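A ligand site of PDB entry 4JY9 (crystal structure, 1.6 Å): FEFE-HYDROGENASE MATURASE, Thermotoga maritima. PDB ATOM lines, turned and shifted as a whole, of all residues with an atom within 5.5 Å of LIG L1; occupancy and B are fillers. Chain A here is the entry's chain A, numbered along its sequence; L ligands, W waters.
An oxygen (O4) of LIG L1 lies within hydrogen-bond range of the side-chain carboxylate (OE2) of Glu 161, 2.4 Å away.
N5 of LIG L1 is in hydrogen-bond range of N of Ile 231 (3.0 Å).
N4 of LIG L1 is in hydrogen-bond range of O of Ile 231, 2.8 Å away.
The backbone carbonyl oxygen of Tyr 69 sits at hydrogen-bond distance from a nitrogen (N4) of LIG L1 (2.9 Å).
O2 of LIG L1 lies within salt-bridge range of NH2 of Arg 180 (3.0 Å).
O of Ser 108 lies close to N1 of LIG L1.
O5 of LIG L1 sits at hydrogen-bond distance from NH1 of Arg 159, 3.1 Å away.
SG of Cys 70 binds FE4 of LG2 L2 (2.3 Å).
The side-chain sulfur (SG) of Cys 63 is bound to an iron atom (FE3) of LG2 L2, at 2.3 Å.
An oxygen (O1) of LIG L1 is bound to an iron atom (FE2) of LG2 L2, at 2.2 Å.
The backbone carbonyl oxygen (O) of Glu 161 sits at hydrogen-bond distance from the backbone NH (N) of Met 199 (3.1 Å).
The backbone carbonyl oxygen of Arg 159 sits at hydrogen-bond distance from the guanidinium group of Arg 180 (2.8 Å).
N of Ser 108 is in hydrogen-bond range of O of Ser 136 (3.3 Å).
OH of Tyr 303 sits at hydrogen-bond distance from OE1 of Gln 107, at 2.9 Å.
The side-chain hydroxyl (OG) of Ser 136 lies within hydrogen-bond range of the side-chain amide nitrogen (NE2) of Gln 107 (3.1 Å).
The backbone carbonyl oxygen (O) of Leu 157 sits at hydrogen-bond distance from the side-chain hydroxyl (OG) of Ser 136.
The backbone NH of Gly 71 sits at hydrogen-bond distance from the backbone carbonyl oxygen of Leu 305 (2.9 Å).
N of Ala 270 lies within hydrogen-bond range of OH of Tyr 306 (3.2 Å).
The side-chain sulfur of Met 199 lies close to a nitrogen (N6) of LIG L1 (3.6 Å).
Cys 70 touches LIG L1.
Gln 107 touches LIG L1 (NE2 to C5, 3.8 Å).
Ser 136 touches LIG L1 (O to C2, 3.5 Å).
N of Gly 138 touches C1 of LIG L1 (3.8 Å).
CD1 of Leu 158 touches O2 of LIG L1, at 3.9 Å.
O of Pro 229 touches C13 of LIG L1 (3.2 Å).
Phe 230 touches LIG L1.
Tyr 303 touches LIG L1 (OH to C3, 3.5 Å).
Leu 305 touches LIG L1 (CD1 to O3, 3.5 Å).
CD2 of Tyr 306 touches C13 of LIG L1, 3.7 Å away.
Hydrophobic or aromatic side chains within 4 Å of LIG L1: Tyr 69, Leu 158, Met 199, Ile 231, Leu 305 and Tyr 306.
17 residues have an atom within 4 Å of LIG L1: Tyr 69, Cys 70, Gln 107, Ser 108, Ser 136, Gly 138, Leu 158, Arg 159, Glu 161, Arg 180, Met 199, Pro 229, Phe 230, Ile 231, Tyr 303, Leu 305 and Tyr 306.
Water W5 bridges an oxygen (O4) of LIG L1 (2.7 Å) and the backbone NH (N) of Arg 159 (3.0 Å).
Water W2 lies within hydrogen-bond range of O of Leu 157 (2.7 Å), O2 of LIG L1 (2.8 Å), N of Gly 138 (3.0 Å), OG of Ser 136 (3.1 Å) and N of Leu 137 (3.3 Å).
Water W4 lies within hydrogen-bond range of the guanidinium group (NH1) of Arg 159 and a nitrogen (N6) of LIG L1.
Water W1 lies within hydrogen-bond range of the side-chain carboxylate (OE2) of Glu 110 (2.7 Å), the guanidinium group (NH1) of Arg 180 (2.7 Å), the guanidinium group (NH2) of Arg 172 (3.3 Å) and a sulfur (S4) of LG2 L2 (3.3 Å).
Water W6 lies within hydrogen-bond range of OH of Tyr 69 (2.7 Å), OE2 of Glu 161 (2.8 Å), NE of Arg 172 (3.1 Å) and S3 of LG2 L2 (3.2 Å).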
ATOM      1  N   CYS A  63     -22.857  -2.704  18.871  1.00  0.00           N
ATOM      2  CA  CYS A  63     -22.504  -2.729  20.259  1.00  0.00           C
ATOM      3  C   CYS A  63     -21.983  -1.417  20.771  1.00  0.00           C
ATOM      4  O   CYS A  63     -21.245  -0.711  20.076  1.00  0.00           O
ATOM      5  CB  CYS A  63     -21.443  -3.805  20.536  1.00  0.00           C
ATOM      6  SG  CYS A  63     -21.333  -4.205  22.302  1.00  0.00           S
ATOM      7  N   TYR A  69     -11.104  -7.909  22.964  1.00  0.00           N
ATOM      8  CA  TYR A  69     -11.043  -9.172  22.201  1.00  0.00           C
ATOM      9  C   TYR A  69     -12.021  -9.294  21.054  1.00  0.00           C
ATOM     10  O   TYR A  69     -11.842 -10.135  20.140  1.00  0.00           O
ATOM     11  CB  TYR A  69     -11.195 -10.394  23.128  1.00  0.00           C
ATOM     12  CG  TYR A  69     -12.343 -10.283  24.070  1.00  0.00           C
ATOM     13  CD1 TYR A  69     -13.651 -10.529  23.664  1.00  0.00           C
ATOM     14  CD2 TYR A  69     -12.127  -9.897  25.402  1.00  0.00           C
ATOM     15  CE1 TYR A  69     -14.677 -10.398  24.565  1.00  0.00           C
ATOM     16  CE2 TYR A  69     -13.171  -9.711  26.301  1.00  0.00           C
ATOM     17  CZ  TYR A  69     -14.433 -10.003  25.873  1.00  0.00           C
ATOM     18  OH  TYR A  69     -15.445  -9.849  26.797  1.00  0.00           O
ATOM     19  N   CYS A  70     -13.054  -8.446  21.065  1.00  0.00           N
ATOM     20  CA  CYS A  70     -14.262  -8.708  20.241  1.00  0.00           C
ATOM     21  C   CYS A  70     -14.336  -7.884  18.957  1.00  0.00           C
ATOM     22  O   CYS A  70     -14.210  -6.676  18.990  1.00  0.00           O
ATOM     23  CB  CYS A  70     -15.488  -8.386  21.081  1.00  0.00           C
ATOM     24  SG  CYS A  70     -17.045  -8.852  20.266  1.00  0.00           S
ATOM     25  N   GLY A  71     -14.580  -8.541  17.823  1.00  0.00           N
ATOM     26  CA  GLY A  71     -14.747  -7.901  16.574  1.00  0.00           C
ATOM     27  C   GLY A  71     -15.933  -6.955  16.478  1.00  0.00           C
ATOM     28  O   GLY A  71     -15.922  -6.048  15.648  1.00  0.00           O
ATOM     29  N   GLN A 107     -29.182 -13.570  20.441  1.00  0.00           N
ATOM     30  CA  GLN A 107     -27.877 -13.011  20.840  1.00  0.00           C
ATOM     31  C   GLN A 107     -27.603 -11.764  20.023  1.00  0.00           C
ATOM     32  O   GLN A 107     -27.940 -11.688  18.859  1.00  0.00           O
ATOM     33  CB  GLN A 107     -26.748 -13.994  20.649  1.00  0.00           C
ATOM     34  CG  GLN A 107     -25.437 -13.521  21.256  1.00  0.00           C
ATOM     35  CD  GLN A 107     -24.344 -14.515  21.125  1.00  0.00           C
ATOM     36  OE1 GLN A 107     -23.667 -14.524  20.104  1.00  0.00           O
ATOM     37  NE2 GLN A 107     -24.084 -15.309  22.199  1.00  0.00           N
ATOM     38  N   SER A 108     -26.960 -10.793  20.651  1.00  0.00           N
ATOM     39  CA  SER A 108     -26.587  -9.564  19.972  1.00  0.00           C
ATOM     40  C   SER A 108     -25.415  -8.884  20.677  1.00  0.00           C
ATOM     41  O   SER A 108     -25.035  -9.199  21.840  1.00  0.00           O
ATOM     42  CB  SER A 108     -27.757  -8.602  19.910  1.00  0.00           C
ATOM     43  OG  SER A 108     -28.195  -8.213  21.219  1.00  0.00           O
ATOM     44  N   GLY A 109     -24.847  -7.922  19.952  1.00  0.00           N
ATOM     45  CA  GLY A 109     -24.070  -6.883  20.625  1.00  0.00           C
ATOM     46  C   GLY A 109     -24.977  -6.166  21.621  1.00  0.00           C
ATOM     47  O   GLY A 109     -26.218  -6.284  21.581  1.00  0.00           O
ATOM     48  N   GLU A 110     -24.393  -5.375  22.498  1.00  0.00           N
ATOM     49  CA  GLU A 110     -25.181  -4.522  23.414  1.00  0.00           C
ATOM     50  C   GLU A 110     -25.700  -3.344  22.642  1.00  0.00           C
ATOM     51  O   GLU A 110     -25.128  -2.246  22.656  1.00  0.00           O
ATOM     52  CB  GLU A 110     -24.361  -4.102  24.629  1.00  0.00           C
ATOM     53  CG  GLU A 110     -23.954  -5.252  25.561  1.00  0.00           C
ATOM     54  CD  GLU A 110     -23.516  -4.762  26.939  1.00  0.00           C
ATOM     55  OE1 GLU A 110     -23.541  -3.522  27.202  1.00  0.00           O
ATOM     56  OE2 GLU A 110     -23.128  -5.648  27.736  1.00  0.00           O
ATOM     57  N   SER A 136     -29.103 -13.623  25.223  1.00  0.00           N
ATOM     58  CA  SER A 136     -27.642 -13.381  25.384  1.00  0.00           C
ATOM     59  C   SER A 136     -27.380 -12.005  24.833  1.00  0.00           C
ATOM     60  O   SER A 136     -26.845 -11.832  23.763  1.00  0.00           O
ATOM     61  CB  SER A 136     -26.862 -14.477  24.665  1.00  0.00           C
ATOM     62  OG  SER A 136     -25.498 -14.352  24.828  1.00  0.00           O
ATOM     63  N   LEU A 137     -27.727 -10.992  25.633  1.00  0.00           N
ATOM     64  CA  LEU A 137     -27.734  -9.580  25.195  1.00  0.00           C
ATOM     65  C   LEU A 137     -26.753  -8.732  25.970  1.00  0.00           C
ATOM     66  O   LEU A 137     -26.663  -7.517  25.744  1.00  0.00           O
ATOM     67  CB  LEU A 137     -29.101  -8.986  25.360  1.00  0.00           C
ATOM     68  CG  LEU A 137     -30.266  -9.803  24.872  1.00  0.00           C
ATOM     69  CD1 LEU A 137     -31.639  -9.092  25.085  1.00  0.00           C
ATOM     70  CD2 LEU A 137     -30.105 -10.204  23.381  1.00  0.00           C
ATOM     71  N   GLY A 138     -25.966  -9.335  26.866  1.00  0.00           N
ATOM     72  CA  GLY A 138     -24.981  -8.574  27.632  1.00  0.00           C
ATOM     73  C   GLY A 138     -25.524  -8.017  28.945  1.00  0.00           C
ATOM     74  O   GLY A 138     -26.489  -8.555  29.551  1.00  0.00           O
ATOM     75  N   LEU A 157     -27.684 -16.250  28.893  1.00  0.00           N
ATOM     76  CA  LEU A 157     -26.282 -16.571  28.800  1.00  0.00           C
ATOM     77  C   LEU A 157     -25.460 -15.338  28.921  1.00  0.00           C
ATOM     78  O   LEU A 157     -25.604 -14.404  28.127  1.00  0.00           O
ATOM     79  CB  LEU A 157     -25.972 -17.199  27.440  1.00  0.00           C
ATOM     80  CG  LEU A 157     -26.824 -18.268  26.889  1.00  0.00           C
ATOM     81  CD1 LEU A 157     -26.296 -18.660  25.468  1.00  0.00           C
ATOM     82  CD2 LEU A 157     -26.870 -19.414  27.871  1.00  0.00           C
ATOM     83  N   LEU A 158     -24.589 -15.335  29.923  1.00  0.00           N
ATOM     84  CA  LEU A 158     -23.712 -14.182  30.232  1.00  0.00           C
ATOM     85  C   LEU A 158     -22.363 -14.676  30.679  1.00  0.00           C
ATOM     86  O   LEU A 158     -22.076 -14.827  31.885  1.00  0.00           O
ATOM     87  CB  LEU A 158     -24.351 -13.230  31.245  1.00  0.00           C
ATOM     88  CG  LEU A 158     -23.691 -11.872  31.367  1.00  0.00           C
ATOM     89  CD1 LEU A 158     -23.979 -10.954  30.088  1.00  0.00           C
ATOM     90  CD2 LEU A 158     -24.200 -11.219  32.672  1.00  0.00           C
ATOM     91  N   ARG A 159     -21.557 -15.066  29.701  1.00  0.00           N
ATOM     92  CA  ARG A 159     -20.271 -15.639  30.033  1.00  0.00           C
ATOM     93  C   ARG A 159     -19.522 -14.687  30.971  1.00  0.00           C
ATOM     94  O   ARG A 159     -19.501 -13.463  30.728  1.00  0.00           O
ATOM     95  CB  ARG A 159     -19.450 -15.867  28.784  1.00  0.00           C
ATOM     96  CG  ARG A 159     -19.941 -17.013  27.982  1.00  0.00           C
ATOM     97  CD  ARG A 159     -18.829 -17.258  26.979  1.00  0.00           C
ATOM     98  NE  ARG A 159     -19.242 -18.170  25.998  1.00  0.00           N
ATOM     99  CZ  ARG A 159     -18.523 -18.526  24.963  1.00  0.00           C
ATOM    100  NH1 ARG A 159     -17.311 -17.982  24.835  1.00  0.00           N
ATOM    101  NH2 ARG A 159     -19.061 -19.433  24.119  1.00  0.00           N
ATOM    102  N   GLU A 161     -16.334 -14.558  31.331  1.00  0.00           N
ATOM    103  CA  GLU A 161     -15.163 -14.231  30.449  1.00  0.00           C
ATOM    104  C   GLU A 161     -13.820 -14.587  31.115  1.00  0.00           C
ATOM    105  O   GLU A 161     -13.025 -15.340  30.573  1.00  0.00           O
ATOM    106  CB  GLU A 161     -15.162 -12.777  29.969  1.00  0.00           C
ATOM    107  CG  GLU A 161     -16.502 -12.281  29.453  1.00  0.00           C
ATOM    108  CD  GLU A 161     -17.039 -13.000  28.217  1.00  0.00           C
ATOM    109  OE1 GLU A 161     -16.440 -13.948  27.710  1.00  0.00           O
ATOM    110  OE2 GLU A 161     -18.075 -12.569  27.711  1.00  0.00           O
ATOM    111  N   ARG A 172     -12.161  -5.424  29.339  1.00  0.00           N
ATOM    112  CA  ARG A 172     -13.556  -4.985  29.236  1.00  0.00           C
ATOM    113  C   ARG A 172     -13.679  -3.621  29.931  1.00  0.00           C
ATOM    114  O   ARG A 172     -14.273  -3.474  30.984  1.00  0.00           O
ATOM    115  CB  ARG A 172     -14.491  -6.029  29.761  1.00  0.00           C
ATOM    116  CG  ARG A 172     -14.231  -7.395  29.207  1.00  0.00           C
ATOM    117  CD  ARG A 172     -15.276  -8.432  29.634  1.00  0.00           C
ATOM    118  NE  ARG A 172     -16.538  -8.101  28.972  1.00  0.00           N
ATOM    119  CZ  ARG A 172     -17.643  -7.672  29.572  1.00  0.00           C
ATOM    120  NH1 ARG A 172     -17.757  -7.676  30.893  1.00  0.00           N
ATOM    121  NH2 ARG A 172     -18.667  -7.240  28.820  1.00  0.00           N
ATOM    122  N   ARG A 180     -20.256  -7.797  36.216  1.00  0.00           N
ATOM    123  CA  ARG A 180     -20.614  -9.043  35.498  1.00  0.00           C
ATOM    124  C   ARG A 180     -21.207 -10.056  36.469  1.00  0.00           C
ATOM    125  O   ARG A 180     -22.248 -10.680  36.182  1.00  0.00           O
ATOM    126  CB  ARG A 180     -19.366  -9.612  34.820  1.00  0.00           C
ATOM    127  CG  ARG A 180     -19.635 -10.654  33.760  1.00  0.00           C
ATOM    128  CD  ARG A 180     -20.111  -9.976  32.509  1.00  0.00           C
ATOM    129  NE  ARG A 180     -20.129 -10.848  31.309  1.00  0.00           N
ATOM    130  CZ  ARG A 180     -20.581 -10.466  30.108  1.00  0.00           C
ATOM    131  NH1 ARG A 180     -20.965  -9.226  29.915  1.00  0.00           N
ATOM    132  NH2 ARG A 180     -20.649 -11.307  29.087  1.00  0.00           N
ATOM    133  N   MET A 199     -13.365 -17.549  28.394  1.00  0.00           N
ATOM    134  CA  MET A 199     -12.449 -17.781  27.292  1.00  0.00           C
ATOM    135  C   MET A 199     -11.130 -18.334  27.859  1.00  0.00           C
ATOM    136  O   MET A 199     -10.744 -18.039  28.996  1.00  0.00           O
ATOM    137  CB  MET A 199     -12.188 -16.551  26.483  1.00  0.00           C
ATOM    138  CG  MET A 199     -13.346 -16.130  25.580  1.00  0.00           C
ATOM    139  SD  MET A 199     -13.068 -14.580  24.722  1.00  0.00           S
ATOM    140  CE  MET A 199     -13.403 -13.452  26.053  1.00  0.00           C
ATOM    141  N   PRO A 229     -11.968 -21.129  23.121  1.00  0.00           N
ATOM    142  CA  PRO A 229     -10.670 -20.478  23.028  1.00  0.00           C
ATOM    143  C   PRO A 229     -10.825 -19.033  22.611  1.00  0.00           C
ATOM    144  O   PRO A 229     -11.706 -18.713  21.854  1.00  0.00           O
ATOM    145  CB  PRO A 229      -9.977 -21.242  21.929  1.00  0.00           C
ATOM    146  CG  PRO A 229     -11.129 -21.623  21.047  1.00  0.00           C
ATOM    147  CD  PRO A 229     -12.285 -21.909  21.938  1.00  0.00           C
ATOM    148  N   PHE A 230      -9.953 -18.188  23.114  1.00  0.00           N
ATOM    149  CA  PHE A 230      -9.771 -16.842  22.547  1.00  0.00           C
ATOM    150  C   PHE A 230      -9.256 -16.984  21.111  1.00  0.00           C
ATOM    151  O   PHE A 230      -8.216 -17.646  20.881  1.00  0.00           O
ATOM    152  CB  PHE A 230      -8.786 -16.023  23.423  1.00  0.00           C
ATOM    153  CG  PHE A 230      -8.265 -14.812  22.742  1.00  0.00           C
ATOM    154  CD1 PHE A 230      -9.087 -13.743  22.403  1.00  0.00           C
ATOM    155  CD2 PHE A 230      -6.915 -14.734  22.439  1.00  0.00           C
ATOM    156  CE1 PHE A 230      -8.612 -12.632  21.703  1.00  0.00           C
ATOM    157  CE2 PHE A 230      -6.430 -13.608  21.722  1.00  0.00           C
ATOM    158  CZ  PHE A 230      -7.297 -12.565  21.373  1.00  0.00           C
ATOM    159  N   ILE A 231      -9.893 -16.256  20.199  1.00  0.00           N
ATOM    160  CA  ILE A 231      -9.469 -16.207  18.790  1.00  0.00           C
ATOM    161  C   ILE A 231      -9.223 -14.761  18.387  1.00  0.00           C
ATOM    162  O   ILE A 231     -10.151 -13.962  18.365  1.00  0.00           O
ATOM    163  CB  ILE A 231     -10.490 -16.865  17.815  1.00  0.00           C
ATOM    164  CG1 ILE A 231     -10.770 -18.325  18.223  1.00  0.00           C
ATOM    165  CG2 ILE A 231     -10.043 -16.716  16.358  1.00  0.00           C
ATOM    166  CD1 ILE A 231     -11.929 -18.952  17.482  1.00  0.00           C
ATOM    167  N   PRO A 232      -7.931 -14.390  18.125  1.00  0.00           N
ATOM    168  CA  PRO A 232      -7.649 -12.979  17.823  1.00  0.00           C
ATOM    169  C   PRO A 232      -8.345 -12.462  16.599  1.00  0.00           C
ATOM    170  O   PRO A 232      -8.400 -13.170  15.572  1.00  0.00           O
ATOM    171  CB  PRO A 232      -6.136 -12.921  17.655  1.00  0.00           C
ATOM    172  CG  PRO A 232      -5.736 -14.329  17.466  1.00  0.00           C
ATOM    173  CD  PRO A 232      -6.713 -15.219  18.124  1.00  0.00           C
ATOM    174  N   HIS A 233      -8.849 -11.249  16.676  1.00  0.00           N
ATOM    175  CA  HIS A 233      -9.543 -10.631  15.566  1.00  0.00           C
ATOM    176  C   HIS A 233      -8.653  -9.491  15.054  1.00  0.00           C
ATOM    177  O   HIS A 233      -8.183  -8.661  15.829  1.00  0.00           O
ATOM    178  CB  HIS A 233     -10.881 -10.061  16.050  1.00  0.00           C
ATOM    179  CG  HIS A 233     -11.770  -9.604  14.946  1.00  0.00           C
ATOM    180  ND1 HIS A 233     -11.482  -8.517  14.172  1.00  0.00           N
ATOM    181  CD2 HIS A 233     -12.963 -10.113  14.451  1.00  0.00           C
ATOM    182  CE1 HIS A 233     -12.438  -8.340  13.283  1.00  0.00           C
ATOM    183  NE2 HIS A 233     -13.343  -9.313  13.435  1.00  0.00           N
ATOM    184  N   ALA A 270     -16.568 -21.559  18.581  1.00  0.00           N
ATOM    185  CA  ALA A 270     -15.122 -21.218  18.622  1.00  0.00           C
ATOM    186  C   ALA A 270     -14.269 -22.485  18.643  1.00  0.00           C
ATOM    187  O   ALA A 270     -13.182 -22.523  17.997  1.00  0.00           O
ATOM    188  CB  ALA A 270     -14.772 -20.266  19.763  1.00  0.00           C
ATOM    189  N   TYR A 303     -21.543 -10.996  11.654  1.00  0.00           N
ATOM    190  CA  TYR A 303     -21.500 -11.197  13.108  1.00  0.00           C
ATOM    191  C   TYR A 303     -20.146 -11.806  13.474  1.00  0.00           C
ATOM    192  O   TYR A 303     -20.016 -12.959  13.656  1.00  0.00           O
ATOM    193  CB  TYR A 303     -22.709 -12.005  13.573  1.00  0.00           C
ATOM    194  CG  TYR A 303     -22.894 -11.957  15.055  1.00  0.00           C
ATOM    195  CD1 TYR A 303     -23.599 -10.881  15.661  1.00  0.00           C
ATOM    196  CD2 TYR A 303     -22.367 -12.944  15.890  1.00  0.00           C
ATOM    197  CE1 TYR A 303     -23.818 -10.827  17.014  1.00  0.00           C
ATOM    198  CE2 TYR A 303     -22.597 -12.856  17.243  1.00  0.00           C
ATOM    199  CZ  TYR A 303     -23.303 -11.793  17.796  1.00  0.00           C
ATOM    200  OH  TYR A 303     -23.527 -11.734  19.161  1.00  0.00           O
ATOM    201  N   LEU A 305     -17.468 -11.899  15.720  1.00  0.00           N
ATOM    202  CA  LEU A 305     -16.841 -11.791  17.096  1.00  0.00           C
ATOM    203  C   LEU A 305     -15.344 -12.098  16.919  1.00  0.00           C
ATOM    204  O   LEU A 305     -14.503 -11.468  17.503  1.00  0.00           O
ATOM    205  CB  LEU A 305     -17.456 -12.769  18.104  1.00  0.00           C
ATOM    206  CG  LEU A 305     -18.978 -12.646  18.321  1.00  0.00           C
ATOM    207  CD1 LEU A 305     -19.461 -13.914  19.062  1.00  0.00           C
ATOM    208  CD2 LEU A 305     -19.366 -11.389  19.064  1.00  0.00           C
ATOM    209  N   TYR A 306     -15.070 -13.155  16.134  1.00  0.00           N
ATOM    210  CA  TYR A 306     -13.753 -13.572  15.753  1.00  0.00           C
ATOM    211  C   TYR A 306     -13.787 -13.970  14.296  1.00  0.00           C
ATOM    212  O   TYR A 306     -14.856 -14.320  13.779  1.00  0.00           O
ATOM    213  CB  TYR A 306     -13.262 -14.750  16.634  1.00  0.00           C
ATOM    214  CG  TYR A 306     -14.331 -15.844  16.850  1.00  0.00           C
ATOM    215  CD1 TYR A 306     -14.488 -16.883  15.886  1.00  0.00           C
ATOM    216  CD2 TYR A 306     -15.160 -15.855  17.924  1.00  0.00           C
ATOM    217  CE1 TYR A 306     -15.454 -17.850  16.018  1.00  0.00           C
ATOM    218  CE2 TYR A 306     -16.165 -16.848  18.088  1.00  0.00           C
ATOM    219  CZ  TYR A 306     -16.286 -17.835  17.155  1.00  0.00           C
ATOM    220  OH  TYR A 306     -17.262 -18.759  17.284  1.00  0.00           O
HETATM  221  N1  LIG L   1     -22.717  -8.934  23.812  1.00  0.00           N
HETATM  222  C1  LIG L   1     -23.103 -10.152  24.571  1.00  0.00           C
HETATM  223  C2  LIG L   1     -23.357 -11.329  23.657  1.00  0.00           C
HETATM  224  C3  LIG L   1     -22.444 -11.388  22.442  1.00  0.00           C
HETATM  225  S1  LIG L   1     -20.715 -11.698  22.738  1.00  0.00           S
HETATM  226  C4  LIG L   1     -22.044 -10.430  25.642  1.00  0.00           C
HETATM  227  O1  LIG L   1     -20.890  -9.845  25.596  1.00  0.00           O
HETATM  228  O2  LIG L   1     -22.273 -11.210  26.561  1.00  0.00           O
HETATM  229  C5  LIG L   1     -20.775 -13.531  22.945  1.00  0.00           C
HETATM  230  C6  LIG L   1     -19.497 -14.234  23.510  1.00  0.00           C
HETATM  231  O3  LIG L   1     -18.530 -14.256  22.451  1.00  0.00           O
HETATM  232  C7  LIG L   1     -18.721 -13.536  24.631  1.00  0.00           C
HETATM  233  O4  LIG L   1     -19.228 -13.749  25.904  1.00  0.00           O
HETATM  234  C8  LIG L   1     -17.259 -13.987  24.437  1.00  0.00           C
HETATM  235  O5  LIG L   1     -16.866 -14.997  25.373  1.00  0.00           O
HETATM  236  C9  LIG L   1     -17.233 -14.572  22.987  1.00  0.00           C
HETATM  237  N2  LIG L   1     -16.204 -13.888  22.168  1.00  0.00           N
HETATM  238  C10 LIG L   1     -16.141 -12.545  21.888  1.00  0.00           C
HETATM  239  N3  LIG L   1     -15.025 -12.280  21.180  1.00  0.00           N
HETATM  240  C11 LIG L   1     -14.301 -13.451  21.106  1.00  0.00           C
HETATM  241  C12 LIG L   1     -13.051 -13.866  20.500  1.00  0.00           C
HETATM  242  N4  LIG L   1     -12.267 -12.951  19.927  1.00  0.00           N
HETATM  243  N5  LIG L   1     -12.649 -15.174  20.643  1.00  0.00           N
HETATM  244  C13 LIG L   1     -13.457 -16.113  21.230  1.00  0.00           C
HETATM  245  N6  LIG L   1     -14.657 -15.802  21.746  1.00  0.00           N
HETATM  246  C14 LIG L   1     -15.083 -14.510  21.735  1.00  0.00           C
HETATM  247 FE1  LG2 L   2     -18.165  -6.977  24.370  1.00  0.00          FE
HETATM  248 FE2  LG2 L   2     -20.430  -8.633  23.784  1.00  0.00          FE
HETATM  249 FE3  LG2 L   2     -20.031  -6.036  22.639  1.00  0.00          FE
HETATM  250 FE4  LG2 L   2     -18.422  -8.035  21.869  1.00  0.00          FE
HETATM  251  S1  LG2 L   2     -20.643  -7.959  21.513  1.00  0.00           S
HETATM  252  S2  LG2 L   2     -17.806  -5.854  22.373  1.00  0.00           S
HETATM  253  S3  LG2 L   2     -18.197  -9.248  23.821  1.00  0.00           S
HETATM  254  S4  LG2 L   2     -20.311  -6.541  24.873  1.00  0.00           S
HETATM  255  O   HOH W   1     -21.640  -7.846  27.647  1.00  0.00           O
HETATM  256  O   HOH W   2     -24.904 -12.121  26.870  1.00  0.00           O
HETATM  257  O   HOH W   3     -19.540 -16.862  21.259  1.00  0.00           O
HETATM  258  O   HOH W   4     -15.265 -18.486  22.804  1.00  0.00           O
HETATM  259  O   HOH W   5     -21.721 -13.999  26.888  1.00  0.00           O
HETATM  260  O   HOH W   6     -18.172  -9.890  26.990  1.00  0.00           O
